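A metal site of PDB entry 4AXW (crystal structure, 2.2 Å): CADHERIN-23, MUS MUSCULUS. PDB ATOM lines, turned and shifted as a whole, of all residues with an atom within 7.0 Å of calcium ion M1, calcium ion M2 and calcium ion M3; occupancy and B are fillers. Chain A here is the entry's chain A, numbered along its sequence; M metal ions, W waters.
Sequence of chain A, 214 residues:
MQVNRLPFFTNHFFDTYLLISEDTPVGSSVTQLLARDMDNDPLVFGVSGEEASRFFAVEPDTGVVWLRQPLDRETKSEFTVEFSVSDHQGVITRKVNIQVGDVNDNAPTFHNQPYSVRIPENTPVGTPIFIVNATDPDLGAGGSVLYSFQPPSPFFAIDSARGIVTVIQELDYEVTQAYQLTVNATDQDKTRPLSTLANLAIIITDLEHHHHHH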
ATOM      1  N   GLU A  22      21.462   4.735 -13.965  1.00  0.00           N
ATOM      2  CA  GLU A  22      20.097   5.194 -14.150  1.00  0.00           C
ATOM      3  C   GLU A  22      19.389   5.483 -12.836  1.00  0.00           C
ATOM      4  O   GLU A  22      18.329   6.095 -12.851  1.00  0.00           O
ATOM      5  CB  GLU A  22      19.256   4.231 -15.000  1.00  0.00           C
ATOM      6  CG  GLU A  22      18.902   2.911 -14.339  1.00  0.00           C
ATOM      7  CD  GLU A  22      17.947   2.051 -15.174  1.00  0.00           C
ATOM      8  OE1 GLU A  22      17.060   2.645 -15.815  1.00  0.00           O
ATOM      9  OE2 GLU A  22      18.045   0.793 -15.133  1.00  0.00           O
ATOM     10  N   LEU A  71      16.985   9.561 -15.402  1.00  0.00           N
ATOM     11  CA  LEU A  71      17.457   8.796 -16.522  1.00  0.00           C
ATOM     12  C   LEU A  71      16.692   7.451 -16.516  1.00  0.00           C
ATOM     13  O   LEU A  71      16.142   7.081 -15.496  1.00  0.00           O
ATOM     14  CB  LEU A  71      18.969   8.571 -16.438  1.00  0.00           C
ATOM     15  CG  LEU A  71      19.975   9.724 -16.567  1.00  0.00           C
ATOM     16  CD1 LEU A  71      21.362   9.235 -16.179  1.00  0.00           C
ATOM     17  CD2 LEU A  71      20.040  10.353 -17.972  1.00  0.00           C
ATOM     18  N   ASP A  72      16.591   6.783 -17.650  1.00  0.00           N
ATOM     19  CA  ASP A  72      15.984   5.434 -17.719  1.00  0.00           C
ATOM     20  C   ASP A  72      16.638   4.692 -18.864  1.00  0.00           C
ATOM     21  O   ASP A  72      16.310   4.953 -19.996  1.00  0.00           O
ATOM     22  CB  ASP A  72      14.463   5.509 -17.953  1.00  0.00           C
ATOM     23  CG  ASP A  72      13.802   4.104 -18.086  1.00  0.00           C
ATOM     24  OD1 ASP A  72      14.458   3.076 -17.794  1.00  0.00           O
ATOM     25  OD2 ASP A  72      12.613   4.021 -18.477  1.00  0.00           O
ATOM     26  N   ARG A  73      17.571   3.780 -18.538  1.00  0.00           N
ATOM     27  CA  ARG A  73      18.383   3.037 -19.509  1.00  0.00           C
ATOM     28  C   ARG A  73      17.532   2.216 -20.508  1.00  0.00           C
ATOM     29  O   ARG A  73      17.929   2.033 -21.654  1.00  0.00           O
ATOM     30  CB  ARG A  73      19.302   2.059 -18.773  1.00  0.00           C
ATOM     31  CG  ARG A  73      20.368   1.399 -19.723  1.00  0.00           C
ATOM     32  CD  ARG A  73      20.856   0.031 -19.274  1.00  0.00           C
ATOM     33  NE  ARG A  73      19.785  -0.994 -19.253  1.00  0.00           N
ATOM     34  CZ  ARG A  73      19.381  -1.701 -20.295  1.00  0.00           C
ATOM     35  NH1 ARG A  73      19.987  -1.556 -21.431  1.00  0.00           N
ATOM     36  NH2 ARG A  73      18.393  -2.598 -20.219  1.00  0.00           N
ATOM     37  N   GLU A  74      16.399   1.705 -20.050  1.00  0.00           N
ATOM     38  CA  GLU A  74      15.492   0.960 -20.895  1.00  0.00           C
ATOM     39  C   GLU A  74      14.809   1.852 -21.952  1.00  0.00           C
ATOM     40  O   GLU A  74      14.278   1.324 -22.946  1.00  0.00           O
ATOM     41  CB  GLU A  74      14.415   0.266 -20.050  1.00  0.00           C
ATOM     42  CG  GLU A  74      14.907  -0.971 -19.270  1.00  0.00           C
ATOM     43  CD  GLU A  74      15.888  -0.692 -18.094  1.00  0.00           C
ATOM     44  OE1 GLU A  74      15.655   0.194 -17.242  1.00  0.00           O
ATOM     45  OE2 GLU A  74      16.877  -1.428 -17.958  1.00  0.00           O
ATOM     46  N   THR A  75      14.808   3.166 -21.723  1.00  0.00           N
ATOM     47  CA  THR A  75      14.116   4.123 -22.584  1.00  0.00           C
ATOM     48  C   THR A  75      15.107   4.844 -23.471  1.00  0.00           C
ATOM     49  O   THR A  75      14.807   5.074 -24.615  1.00  0.00           O
ATOM     50  CB  THR A  75      13.326   5.188 -21.778  1.00  0.00           C
ATOM     51  OG1 THR A  75      12.075   4.629 -21.341  1.00  0.00           O
ATOM     52  CG2 THR A  75      13.050   6.435 -22.629  1.00  0.00           C
ATOM     53  N   GLY A 101      24.131   3.616 -16.935  1.00  0.00           N
ATOM     54  CA  GLY A 101      24.278   2.349 -16.230  1.00  0.00           C
ATOM     55  C   GLY A 101      22.952   1.728 -15.827  1.00  0.00           C
ATOM     56  O   GLY A 101      22.036   2.415 -15.397  1.00  0.00           O
ATOM     57  N   ASP A 102      22.867   0.411 -15.925  1.00  0.00           N
ATOM     58  CA  ASP A 102      21.683  -0.323 -15.516  1.00  0.00           C
ATOM     59  C   ASP A 102      21.593  -0.520 -14.037  1.00  0.00           C
ATOM     60  O   ASP A 102      22.622  -0.807 -13.372  1.00  0.00           O
ATOM     61  CB  ASP A 102      21.666  -1.687 -16.171  1.00  0.00           C
ATOM     62  CG  ASP A 102      20.269  -2.330 -16.129  1.00  0.00           C
ATOM     63  OD1 ASP A 102      19.259  -1.672 -16.562  1.00  0.00           O
ATOM     64  OD2 ASP A 102      20.196  -3.486 -15.640  1.00  0.00           O
ATOM     65  N   VAL A 103      20.362  -0.448 -13.522  1.00  0.00           N
ATOM     66  CA  VAL A 103      20.000  -1.154 -12.315  1.00  0.00           C
ATOM     67  C   VAL A 103      18.781  -2.066 -12.570  1.00  0.00           C
ATOM     68  O   VAL A 103      18.051  -1.917 -13.555  1.00  0.00           O
ATOM     69  CB  VAL A 103      19.730  -0.191 -11.107  1.00  0.00           C
ATOM     70  CG1 VAL A 103      20.898   0.846 -10.903  1.00  0.00           C
ATOM     71  CG2 VAL A 103      18.390   0.528 -11.221  1.00  0.00           C
ATOM     72  N   ASN A 104      18.567  -3.037 -11.691  1.00  0.00           N
ATOM     73  CA  ASN A 104      17.400  -3.882 -11.821  1.00  0.00           C
ATOM     74  C   ASN A 104      16.175  -3.087 -11.372  1.00  0.00           C
ATOM     75  O   ASN A 104      15.957  -2.939 -10.188  1.00  0.00           O
ATOM     76  CB  ASN A 104      17.556  -5.170 -11.028  1.00  0.00           C
ATOM     77  CG  ASN A 104      16.429  -6.132 -11.311  1.00  0.00           C
ATOM     78  OD1 ASN A 104      16.061  -6.372 -12.503  1.00  0.00           O
ATOM     79  ND2 ASN A 104      15.826  -6.667 -10.232  1.00  0.00           N
ATOM     80  N   ASP A 105      15.424  -2.504 -12.297  1.00  0.00           N
ATOM     81  CA  ASP A 105      14.205  -1.781 -11.904  1.00  0.00           C
ATOM     82  C   ASP A 105      12.986  -2.245 -12.645  1.00  0.00           C
ATOM     83  O   ASP A 105      11.961  -1.569 -12.585  1.00  0.00           O
ATOM     84  CB  ASP A 105      14.348  -0.262 -12.044  1.00  0.00           C
ATOM     85  CG  ASP A 105      14.925   0.204 -13.435  1.00  0.00           C
ATOM     86  OD1 ASP A 105      15.310  -0.616 -14.328  1.00  0.00           O
ATOM     87  OD2 ASP A 105      15.067   1.443 -13.582  1.00  0.00           O
ATOM     88  N   ASN A 106      13.053  -3.378 -13.330  1.00  0.00           N
ATOM     89  CA  ASN A 106      11.847  -3.959 -13.901  1.00  0.00           C
ATOM     90  C   ASN A 106      11.561  -5.320 -13.393  1.00  0.00           C
ATOM     91  O   ASN A 106      12.484  -6.117 -13.190  1.00  0.00           O
ATOM     92  CB  ASN A 106      11.956  -4.002 -15.411  1.00  0.00           C
ATOM     93  CG  ASN A 106      12.018  -2.630 -16.028  1.00  0.00           C
ATOM     94  OD1 ASN A 106      11.033  -2.163 -16.542  1.00  0.00           O
ATOM     95  ND2 ASN A 106      13.179  -1.953 -15.916  1.00  0.00           N
ATOM     96  N   ALA A 107      10.281  -5.620 -13.238  1.00  0.00           N
ATOM     97  CA  ALA A 107       9.868  -7.010 -12.996  1.00  0.00           C
ATOM     98  C   ALA A 107       9.575  -7.698 -14.331  1.00  0.00           C
ATOM     99  O   ALA A 107       9.312  -7.019 -15.321  1.00  0.00           O
ATOM    100  CB  ALA A 107       8.629  -7.003 -12.106  1.00  0.00           C
ATOM    101  N   PRO A 108       9.573  -9.041 -14.365  1.00  0.00           N
ATOM    102  CA  PRO A 108       9.143  -9.744 -15.608  1.00  0.00           C
ATOM    103  C   PRO A 108       7.699  -9.501 -16.043  1.00  0.00           C
ATOM    104  O   PRO A 108       6.862  -9.205 -15.207  1.00  0.00           O
ATOM    105  CB  PRO A 108       9.350 -11.225 -15.308  1.00  0.00           C
ATOM    106  CG  PRO A 108      10.245 -11.270 -14.113  1.00  0.00           C
ATOM    107  CD  PRO A 108      10.057  -9.993 -13.339  1.00  0.00           C
ATOM    108  N   ASP A 136      12.055  -9.833 -19.378  1.00  0.00           N
ATOM    109  CA  ASP A 136      12.476  -8.820 -18.401  1.00  0.00           C
ATOM    110  C   ASP A 136      13.585  -8.025 -19.075  1.00  0.00           C
ATOM    111  O   ASP A 136      14.586  -8.596 -19.443  1.00  0.00           O
ATOM    112  CB  ASP A 136      12.979  -9.495 -17.109  1.00  0.00           C
ATOM    113  CG  ASP A 136      13.276  -8.505 -15.993  1.00  0.00           C
ATOM    114  OD1 ASP A 136      13.907  -7.444 -16.285  1.00  0.00           O
ATOM    115  OD2 ASP A 136      12.972  -8.824 -14.809  1.00  0.00           O
ATOM    116  N   PRO A 137      13.424  -6.712 -19.244  1.00  0.00           N
ATOM    117  CA  PRO A 137      14.384  -5.950 -20.065  1.00  0.00           C
ATOM    118  C   PRO A 137      15.654  -5.435 -19.337  1.00  0.00           C
ATOM    119  O   PRO A 137      16.492  -4.803 -19.978  1.00  0.00           O
ATOM    120  CB  PRO A 137      13.556  -4.747 -20.523  1.00  0.00           C
ATOM    121  CG  PRO A 137      12.744  -4.445 -19.274  1.00  0.00           C
ATOM    122  CD  PRO A 137      12.414  -5.845 -18.658  1.00  0.00           C
ATOM    123  N   ASP A 138      15.800  -5.672 -18.045  1.00  0.00           N
ATOM    124  CA  ASP A 138      17.032  -5.323 -17.352  1.00  0.00           C
ATOM    125  C   ASP A 138      18.214  -6.153 -17.843  1.00  0.00           C
ATOM    126  O   ASP A 138      18.016  -7.161 -18.492  1.00  0.00           O
ATOM    127  CB  ASP A 138      16.871  -5.496 -15.860  1.00  0.00           C
ATOM    128  CG  ASP A 138      15.772  -4.598 -15.272  1.00  0.00           C
ATOM    129  OD1 ASP A 138      15.924  -3.349 -15.369  1.00  0.00           O
ATOM    130  OD2 ASP A 138      14.793  -5.147 -14.701  1.00  0.00           O
ATOM    131  N   LEU A 139      19.439  -5.728 -17.549  1.00  0.00           N
ATOM    132  CA  LEU A 139      20.623  -6.459 -17.999  1.00  0.00           C
ATOM    133  C   LEU A 139      20.979  -7.569 -17.040  1.00  0.00           C
ATOM    134  O   LEU A 139      20.814  -7.408 -15.816  1.00  0.00           O
ATOM    135  CB  LEU A 139      21.841  -5.518 -18.075  1.00  0.00           C
ATOM    136  CG  LEU A 139      21.774  -4.402 -19.107  1.00  0.00           C
ATOM    137  CD1 LEU A 139      23.114  -3.729 -19.130  1.00  0.00           C
ATOM    138  CD2 LEU A 139      21.370  -4.901 -20.537  1.00  0.00           C
ATOM    139  N   ALA A 141      21.832 -10.824 -14.734  1.00  0.00           N
ATOM    140  CA  ALA A 141      20.962 -11.555 -13.799  1.00  0.00           C
ATOM    141  C   ALA A 141      19.599 -10.887 -13.600  1.00  0.00           C
ATOM    142  O   ALA A 141      18.566 -11.541 -13.477  1.00  0.00           O
ATOM    143  CB  ALA A 141      21.659 -11.746 -12.480  1.00  0.00           C
ATOM    144  N   GLY A 142      19.574  -9.565 -13.653  1.00  0.00           N
ATOM    145  CA  GLY A 142      18.294  -8.853 -13.549  1.00  0.00           C
ATOM    146  C   GLY A 142      17.334  -9.047 -14.703  1.00  0.00           C
ATOM    147  O   GLY A 142      16.204  -8.614 -14.614  1.00  0.00           O
ATOM    148  N   GLY A 143      17.781  -9.694 -15.763  1.00  0.00           N
ATOM    149  CA  GLY A 143      16.923  -9.957 -16.937  1.00  0.00           C
ATOM    150  C   GLY A 143      16.723 -11.442 -17.212  1.00  0.00           C
ATOM    151  O   GLY A 143      16.119 -11.806 -18.181  1.00  0.00           O
ATOM    152  N   SER A 144      17.219 -12.307 -16.345  1.00  0.00           N
ATOM    153  CA  SER A 144      17.128 -13.749 -16.573  1.00  0.00           C
ATOM    154  C   SER A 144      16.029 -14.255 -15.670  1.00  0.00           C
ATOM    155  O   SER A 144      16.127 -14.096 -14.475  1.00  0.00           O
ATOM    156  CB  SER A 144      18.466 -14.395 -16.199  1.00  0.00           C
ATOM    157  OG  SER A 144      18.433 -15.800 -16.388  1.00  0.00           O
ATOM    158  N   THR A 186      10.439 -14.583 -11.591  1.00  0.00           N
ATOM    159  CA  THR A 186      11.341 -13.671 -10.897  1.00  0.00           C
ATOM    160  C   THR A 186      12.600 -13.499 -11.733  1.00  0.00           C
ATOM    161  O   THR A 186      13.038 -14.448 -12.447  1.00  0.00           O
ATOM    162  CB  THR A 186      11.732 -14.204  -9.506  1.00  0.00           C
ATOM    163  OG1 THR A 186      12.673 -13.300  -8.861  1.00  0.00           O
ATOM    164  CG2 THR A 186      12.336 -15.614  -9.592  1.00  0.00           C
ATOM    165  N   ASP A 187      13.172 -12.307 -11.681  1.00  0.00           N
ATOM    166  CA  ASP A 187      14.534 -12.147 -12.122  1.00  0.00           C
ATOM    167  C   ASP A 187      15.481 -12.605 -11.004  1.00  0.00           C
ATOM    168  O   ASP A 187      15.007 -13.028  -9.927  1.00  0.00           O
ATOM    169  CB  ASP A 187      14.852 -10.743 -12.636  1.00  0.00           C
ATOM    170  CG  ASP A 187      14.739  -9.681 -11.588  1.00  0.00           C
ATOM    171  OD1 ASP A 187      15.146  -9.949 -10.435  1.00  0.00           O
ATOM    172  OD2 ASP A 187      14.283  -8.545 -11.951  1.00  0.00           O
ATOM    173  N   GLN A 188      16.794 -12.584 -11.299  1.00  0.00           N
ATOM    174  CA  GLN A 188      17.818 -13.177 -10.423  1.00  0.00           C
ATOM    175  C   GLN A 188      18.813 -12.160  -9.914  1.00  0.00           C
ATOM    176  O   GLN A 188      19.927 -12.497  -9.548  1.00  0.00           O
ATOM    177  CB  GLN A 188      18.577 -14.242 -11.178  1.00  0.00           C
ATOM    178  CG  GLN A 188      17.727 -15.470 -11.520  1.00  0.00           C
ATOM    179  CD  GLN A 188      18.540 -16.588 -12.157  1.00  0.00           C
ATOM    180  OE1 GLN A 188      19.128 -17.428 -11.446  1.00  0.00           O
ATOM    181  NE2 GLN A 188      18.599 -16.593 -13.495  1.00  0.00           N
ATOM    182  N   ASP A 189      18.427 -10.897  -9.911  1.00  0.00           N
ATOM    183  CA  ASP A 189      19.269  -9.857  -9.360  1.00  0.00           C
ATOM    184  C   ASP A 189      19.621 -10.229  -7.928  1.00  0.00           C
ATOM    185  O   ASP A 189      18.736 -10.582  -7.144  1.00  0.00           O
ATOM    186  CB  ASP A 189      18.544  -8.543  -9.326  1.00  0.00           C
ATOM    187  CG  ASP A 189      19.461  -7.390  -8.972  1.00  0.00           C
ATOM    188  OD1 ASP A 189      20.339  -7.005  -9.804  1.00  0.00           O
ATOM    189  OD2 ASP A 189      19.252  -6.819  -7.887  1.00  0.00           O
ATOM    190  N   ARG A 192      18.292  -6.938  -5.173  1.00  0.00           N
ATOM    191  CA  ARG A 192      16.895  -6.565  -5.309  1.00  0.00           C
ATOM    192  C   ARG A 192      16.136  -7.393  -6.379  1.00  0.00           C
ATOM    193  O   ARG A 192      15.626  -6.866  -7.357  1.00  0.00           O
ATOM    194  CB  ARG A 192      16.824  -5.049  -5.608  1.00  0.00           C
ATOM    195  CG  ARG A 192      17.509  -4.169  -4.549  1.00  0.00           C
ATOM    196  CD  ARG A 192      17.454  -2.679  -4.827  1.00  0.00           C
ATOM    197  NE  ARG A 192      16.062  -2.261  -4.952  1.00  0.00           N
ATOM    198  CZ  ARG A 192      15.427  -2.033  -6.097  1.00  0.00           C
ATOM    199  NH1 ARG A 192      16.077  -2.073  -7.261  1.00  0.00           N
ATOM    200  NH2 ARG A 192      14.116  -1.779  -6.064  1.00  0.00           N
ATOM    201  N   PRO A 193      16.003  -8.698  -6.190  1.00  0.00           N
ATOM    202  CA  PRO A 193      15.156  -9.405  -7.166  1.00  0.00           C
ATOM    203  C   PRO A 193      13.698  -8.878  -7.321  1.00  0.00           C
ATOM    204  O   PRO A 193      13.043  -8.518  -6.337  1.00  0.00           O
ATOM    205  CB  PRO A 193      15.127 -10.818  -6.637  1.00  0.00           C
ATOM    206  CG  PRO A 193      15.368 -10.668  -5.126  1.00  0.00           C
ATOM    207  CD  PRO A 193      16.332  -9.520  -5.005  1.00  0.00           C
ATOM    208  N   LEU A 194      13.174  -8.891  -8.538  1.00  0.00           N
ATOM    209  CA  LEU A 194      11.781  -8.472  -8.731  1.00  0.00           C
ATOM    210  C   LEU A 194      10.994  -9.565  -9.403  1.00  0.00           C
ATOM    211  O   LEU A 194      11.538 -10.355 -10.229  1.00  0.00           O
ATOM    212  CB  LEU A 194      11.708  -7.184  -9.575  1.00  0.00           C
ATOM    213  CG  LEU A 194      12.397  -5.935  -8.984  1.00  0.00           C
ATOM    214  CD1 LEU A 194      12.491  -4.842 -10.048  1.00  0.00           C
ATOM    215  CD2 LEU A 194      11.625  -5.403  -7.734  1.00  0.00           C
HETATM  216 CA    CA M   1      14.362  -7.256 -13.835  1.00  0.00          CA
HETATM  217 CA    CA M   2      17.166  -1.276 -15.572  1.00  0.00          CA
HETATM  218 CA    CA M   3      14.851   1.884 -15.949  1.00  0.00          CA
HETATM  219  O   HOH W   1      13.915   3.882 -14.944  1.00  0.00           O
HETATM  220  O   HOH W   2      12.685   1.167 -16.160  1.00  0.00           O
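The side-chain carboxylate (OD1) of Asp 187 sits at hydrogen-bond distance from the backbone NH (N) of Asp 189.
The side-chain carboxylate (OE1) of Glu 22 lies close to the backbone NH (N) of Arg 73, at 3.0 Å.
The backbone NH (N) of Leu 139 lies within hydrogen-bond range of the side-chain carboxylate (OD2) of Asp 102, at 3.0 Å.
NE of Arg 73 lies close to OD1 of Asp 102 (2.8 Å).
The backbone NH of Asp 187 lies within hydrogen-bond range of the backbone carbonyl oxygen of Leu 194 (2.9 Å).
The side-chain amide nitrogen (ND2) of Asn 104 sits at hydrogen-bond distance from the backbone carbonyl oxygen (O) of Arg 192 (2.9 Å).
The side-chain carboxylate (OD2) of Asp 72 sits at hydrogen-bond distance from the side-chain hydroxyl (OG1) of Thr 75 (3.0 Å).
The side-chain carboxylate (OE2) of Glu 74 lies close to the guanidinium group (NH2) of Arg 73 (3.0 Å).
Of the 29 residues printed, 6 come within 4 Å of calcium ion M1.
The nearest printed residue that does not touch calcium ion M1 is Ala 107 (4.4 Å).
Of the 29 residues printed, 6 come within 4 Å of calcium ion M2.
Within 4 Å of calcium ion M3: Glu 22, Asp 72, Glu 74 and Asp 105.
The nearest printed residue that does not touch calcium ion M3 is Asn 106 (4.2 Å).
Calcium ion M1 is bound by OD2 of Asp 187 (2.3 Å), O of Asn 106 (2.3 Å), OD2 of Asp 136 (2.3 Å), OD2 of Asp 138 (2.3 Å), OD1 of Asn 104 (2.3 Å), O of Gly 142 (2.4 Å) and OD1 of Asp 136 (2.5 Å).
OE2 of Glu 22 binds calcium ion M2, 2.3 Å away.
The backbone carbonyl oxygen (O) of Val 103 binds calcium ion M2 (2.3 Å).
OD1 of Asp 105 binds calcium ion M2 (2.3 Å).
OD1 of Asp 102 is bound to calcium ion M2 (2.3 Å).
The side-chain carboxylate (OE2) of Glu 74 binds calcium ion M2, 2.4 Å away.
Calcium ion M2 is bound by the side-chain carboxylate (OD1) of Asp 138 (2.4 Å).
OE1 of Glu 74 binds calcium ion M2, 2.7 Å away.
Calcium ion M3 is bound by the side-chain carboxylate (OD1) of Asp 72.
Calcium ion M3 is bound by the side-chain carboxylate (OE1) of Glu 74, at 2.3 Å.
Calcium ion M3 is bound by water W2.
The side-chain carboxylate (OE1) of Glu 22 binds calcium ion M3, 2.3 Å away.
OD2 of Asp 105 binds calcium ion M3.
Water W1 is bound to calcium ion M3.
Calcium ion M3 has six donor atoms within binding distance.
Slightly farther from calcium ion M3 lies the side-chain carboxylate (OD1) of Asp 105 (3.0 Å).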
